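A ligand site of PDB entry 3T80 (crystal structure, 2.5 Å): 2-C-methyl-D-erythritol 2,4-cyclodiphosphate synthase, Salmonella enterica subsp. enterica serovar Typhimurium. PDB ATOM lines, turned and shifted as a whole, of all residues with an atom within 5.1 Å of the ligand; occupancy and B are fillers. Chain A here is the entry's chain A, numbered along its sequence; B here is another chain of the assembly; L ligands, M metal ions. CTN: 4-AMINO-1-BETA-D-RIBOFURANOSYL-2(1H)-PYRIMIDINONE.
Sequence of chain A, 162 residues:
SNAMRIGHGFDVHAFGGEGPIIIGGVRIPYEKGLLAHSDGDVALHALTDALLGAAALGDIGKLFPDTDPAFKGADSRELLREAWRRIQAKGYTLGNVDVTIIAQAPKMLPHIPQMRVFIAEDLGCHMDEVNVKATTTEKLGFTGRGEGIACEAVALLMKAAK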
ATOM      1  N   ALA A 103      20.904 -12.268  -2.656  1.00  0.00           N
ATOM      2  CA  ALA A 103      20.517 -11.744  -1.322  1.00  0.00           C
ATOM      3  C   ALA A 103      19.240 -12.340  -0.771  1.00  0.00           C
ATOM      4  O   ALA A 103      18.185 -12.308  -1.401  1.00  0.00           O
ATOM      5  CB  ALA A 103      20.377 -10.229  -1.374  1.00  0.00           C
ATOM      6  N   GLN A 104      19.351 -12.828   0.453  1.00  0.00           N
ATOM      7  CA  GLN A 104      18.164 -13.303   1.230  1.00  0.00           C
ATOM      8  C   GLN A 104      17.199 -12.149   1.474  1.00  0.00           C
ATOM      9  O   GLN A 104      15.975 -12.297   1.485  1.00  0.00           O
ATOM     10  CB  GLN A 104      18.598 -13.870   2.581  1.00  0.00           C
ATOM     11  CG  GLN A 104      17.619 -14.880   3.173  1.00  0.00           C
ATOM     12  CD  GLN A 104      17.264 -15.995   2.214  1.00  0.00           C
ATOM     13  OE1 GLN A 104      18.145 -16.593   1.569  1.00  0.00           O
ATOM     14  NE2 GLN A 104      15.970 -16.288   2.112  1.00  0.00           N
ATOM     15  N   ALA A 105      17.817 -10.982   1.605  1.00  0.00           N
ATOM     16  CA  ALA A 105      17.158  -9.732   2.019  1.00  0.00           C
ATOM     17  C   ALA A 105      18.109  -8.529   1.950  1.00  0.00           C
ATOM     18  O   ALA A 105      19.331  -8.688   2.042  1.00  0.00           O
ATOM     19  CB  ALA A 105      16.621  -9.868   3.442  1.00  0.00           C
ATOM     20  N   PRO A 106      17.566  -7.320   1.799  1.00  0.00           N
ATOM     21  CA  PRO A 106      16.178  -7.018   1.622  1.00  0.00           C
ATOM     22  C   PRO A 106      15.691  -7.251   0.209  1.00  0.00           C
ATOM     23  O   PRO A 106      16.429  -7.718  -0.672  1.00  0.00           O
ATOM     24  CB  PRO A 106      16.147  -5.525   1.920  1.00  0.00           C
ATOM     25  CG  PRO A 106      17.411  -5.042   1.361  1.00  0.00           C
ATOM     26  CD  PRO A 106      18.386  -6.095   1.758  1.00  0.00           C
ATOM     27  N   LYS A 107      14.434  -6.893   0.036  1.00  0.00           N
ATOM     28  CA  LYS A 107      13.688  -7.035  -1.229  1.00  0.00           C
ATOM     29  C   LYS A 107      14.235  -6.046  -2.271  1.00  0.00           C
ATOM     30  O   LYS A 107      14.167  -4.834  -2.102  1.00  0.00           O
ATOM     31  CB  LYS A 107      12.178  -6.823  -1.051  1.00  0.00           C
ATOM     32  N   MET A 108      14.759  -6.604  -3.341  1.00  0.00           N
ATOM     33  CA  MET A 108      15.386  -5.802  -4.426  1.00  0.00           C
ATOM     34  C   MET A 108      14.349  -5.378  -5.463  1.00  0.00           C
ATOM     35  O   MET A 108      14.480  -4.347  -6.104  1.00  0.00           O
ATOM     36  CB  MET A 108      16.499  -6.568  -5.130  1.00  0.00           C
ATOM     37  CG  MET A 108      17.611  -6.983  -4.197  1.00  0.00           C
ATOM     38  SD  MET A 108      18.512  -5.616  -3.419  1.00  0.00           S
ATOM     39  CE  MET A 108      19.372  -6.473  -2.101  1.00  0.00           C
ATOM     40  N   LEU A 109      13.322  -6.198  -5.561  1.00  0.00           N
ATOM     41  CA  LEU A 109      12.284  -6.084  -6.644  1.00  0.00           C
ATOM     42  C   LEU A 109      11.829  -4.661  -6.922  1.00  0.00           C
ATOM     43  O   LEU A 109      11.950  -4.176  -8.048  1.00  0.00           O
ATOM     44  CB  LEU A 109      11.062  -6.955  -6.383  1.00  0.00           C
ATOM     45  CG  LEU A 109      10.055  -6.904  -7.552  1.00  0.00           C
ATOM     46  CD1 LEU A 109      10.612  -7.593  -8.795  1.00  0.00           C
ATOM     47  CD2 LEU A 109       8.708  -7.511  -7.175  1.00  0.00           C
ATOM     48  N   PRO A 110      11.304  -3.964  -5.905  1.00  0.00           N
ATOM     49  CA  PRO A 110      10.769  -2.638  -6.156  1.00  0.00           C
ATOM     50  C   PRO A 110      11.810  -1.611  -6.644  1.00  0.00           C
ATOM     51  O   PRO A 110      11.450  -0.605  -7.273  1.00  0.00           O
ATOM     52  CB  PRO A 110      10.201  -2.220  -4.812  1.00  0.00           C
ATOM     53  CG  PRO A 110      10.574  -3.237  -3.827  1.00  0.00           C
ATOM     54  CD  PRO A 110      11.301  -4.329  -4.483  1.00  0.00           C
ATOM     55  N   ALA A 134      17.298 -10.458  -9.418  1.00  0.00           N
ATOM     56  CA  ALA A 134      17.550 -10.759  -8.044  1.00  0.00           C
ATOM     57  C   ALA A 134      17.095 -12.143  -7.729  1.00  0.00           C
ATOM     58  O   ALA A 134      16.084 -12.644  -8.242  1.00  0.00           O
ATOM     59  CB  ALA A 134      16.855  -9.771  -7.123  1.00  0.00           C
ATOM     60  N   THR A 135      17.888 -12.748  -6.872  1.00  0.00           N
ATOM     61  CA  THR A 135      17.578 -14.059  -6.372  1.00  0.00           C
ATOM     62  C   THR A 135      18.086 -14.276  -4.960  1.00  0.00           C
ATOM     63  O   THR A 135      18.910 -13.531  -4.435  1.00  0.00           O
ATOM     64  CB  THR A 135      18.087 -15.169  -7.286  1.00  0.00           C
ATOM     65  OG1 THR A 135      17.670 -16.431  -6.746  1.00  0.00           O
ATOM     66  CG2 THR A 135      19.596 -15.149  -7.385  1.00  0.00           C
ATOM     67  N   THR A 136      17.545 -15.305  -4.358  1.00  0.00           N
ATOM     68  CA  THR A 136      18.038 -15.770  -3.057  1.00  0.00           C
ATOM     69  C   THR A 136      18.604 -17.166  -3.193  1.00  0.00           C
ATOM     70  O   THR A 136      18.324 -17.881  -4.141  1.00  0.00           O
ATOM     71  CB  THR A 136      16.961 -15.851  -1.962  1.00  0.00           C
ATOM     72  OG1 THR A 136      16.210 -17.052  -2.152  1.00  0.00           O
ATOM     73  CG2 THR A 136      16.050 -14.650  -1.982  1.00  0.00           C
ATOM     74  N   ASP B  59      13.520 -11.451 -14.969  1.00  0.00           N
ATOM     75  CA  ASP B  59      13.735 -12.825 -14.519  1.00  0.00           C
ATOM     76  C   ASP B  59      12.417 -13.579 -14.510  1.00  0.00           C
ATOM     77  O   ASP B  59      11.414 -13.084 -15.029  1.00  0.00           O
ATOM     78  CB  ASP B  59      14.407 -12.864 -13.137  1.00  0.00           C
ATOM     79  CG  ASP B  59      13.532 -12.274 -12.050  1.00  0.00           C
ATOM     80  OD1 ASP B  59      12.308 -12.158 -12.276  1.00  0.00           O
ATOM     81  OD2 ASP B  59      14.052 -11.925 -10.971  1.00  0.00           O
ATOM     82  N   GLY B  61      10.269 -14.904 -11.879  1.00  0.00           N
ATOM     83  CA  GLY B  61       9.252 -14.323 -10.961  1.00  0.00           C
ATOM     84  C   GLY B  61       8.521 -13.154 -11.601  1.00  0.00           C
ATOM     85  O   GLY B  61       7.573 -12.588 -11.076  1.00  0.00           O
ATOM     86  N   LYS B  62       8.990 -12.809 -12.778  1.00  0.00           N
ATOM     87  CA  LYS B  62       8.399 -11.714 -13.544  1.00  0.00           C
ATOM     88  C   LYS B  62       7.454 -12.274 -14.569  1.00  0.00           C
ATOM     89  O   LYS B  62       6.996 -11.589 -15.492  1.00  0.00           O
ATOM     90  CB  LYS B  62       9.468 -10.909 -14.253  1.00  0.00           C
ATOM     91  CG  LYS B  62       9.058  -9.490 -14.581  1.00  0.00           C
ATOM     92  CD  LYS B  62       9.666  -8.527 -13.584  1.00  0.00           C
ATOM     93  CE  LYS B  62       9.532  -7.097 -14.081  1.00  0.00           C
ATOM     94  NZ  LYS B  62       9.880  -6.949 -15.522  1.00  0.00           N
HETATM   95  O5' CTN L   1      13.766 -15.230  -6.605  1.00  0.00           O
HETATM   96  C5' CTN L   1      12.468 -14.963  -6.057  1.00  0.00           C
HETATM   97  C4' CTN L   1      11.949 -13.615  -6.511  1.00  0.00           C
HETATM   98  O4' CTN L   1      12.028 -12.705  -5.428  1.00  0.00           O
HETATM   99  C1' CTN L   1      12.576 -11.462  -5.831  1.00  0.00           C
HETATM  100  N1  CTN L   1      13.692 -11.176  -4.965  1.00  0.00           N
HETATM  101  C6  CTN L   1      14.515 -12.153  -4.612  1.00  0.00           C
HETATM  102  C5  CTN L   1      15.550 -11.873  -3.749  1.00  0.00           C
HETATM  103  C4  CTN L   1      15.682 -10.582  -3.258  1.00  0.00           C
HETATM  104  N3  CTN L   1      14.840  -9.617  -3.606  1.00  0.00           N
HETATM  105  C2  CTN L   1      13.842  -9.884  -4.445  1.00  0.00           C
HETATM  106  O2  CTN L   1      13.055  -8.983  -4.757  1.00  0.00           O
HETATM  107  N4  CTN L   1      16.677 -10.302  -2.418  1.00  0.00           N
HETATM  108  C2' CTN L   1      12.985 -11.602  -7.257  1.00  0.00           C
HETATM  109  O2' CTN L   1      12.050 -10.824  -8.024  1.00  0.00           O
HETATM  110  C3' CTN L   1      12.779 -13.036  -7.633  1.00  0.00           C
HETATM  111  O3' CTN L   1      12.080 -13.079  -8.884  1.00  0.00           O
HETATM  112 MG    MG M   1      15.149 -19.351  -6.186  1.00  0.00          MG
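O3' of the ligand lies within hydrogen-bond range of OD2 of Asp 59 of chain B.
The backbone NH (N) of Met 108 lies within hydrogen-bond range of a nitrogen (N3) of the ligand, at 3.0 Å.
An oxygen (O2) of the ligand lies within hydrogen-bond range of the backbone NH (N) of Leu 109, at 2.9 Å.
A nitrogen (N4) of the ligand sits at hydrogen-bond distance from the backbone carbonyl oxygen (O) of Pro 106, at 3.1 Å.
N4 of the ligand is in hydrogen-bond range of O of Ala 103 (2.7 Å).
The backbone NH (N) of Ala 103 lies within hydrogen-bond range of the backbone carbonyl oxygen (O) of Thr 135 (3.0 Å).
The backbone NH of Lys 62 of chain B is in hydrogen-bond range of the side-chain carboxylate of Asp 59 of chain B (3.4 Å).
N of Gly 61 of chain B is in hydrogen-bond range of OD1 of Asp 59 of chain B, 3.4 Å away.
CA of Lys 107 touches N3 of the ligand (3.7 Å).
Ala 134 touches the ligand.
C of Thr 135 touches C5 of the ligand (3.7 Å).
Thr 136 touches the ligand.
Gly 61 of chain B touches the ligand (CA to O3', 3.7 Å).
Ten residues have an atom within 4 Å of the ligand: Ala 103, Pro 106, Lys 107, Met 108, Leu 109, Ala 134, Thr 135, Thr 136, Asp 59 of chain B and Gly 61 of chain B.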
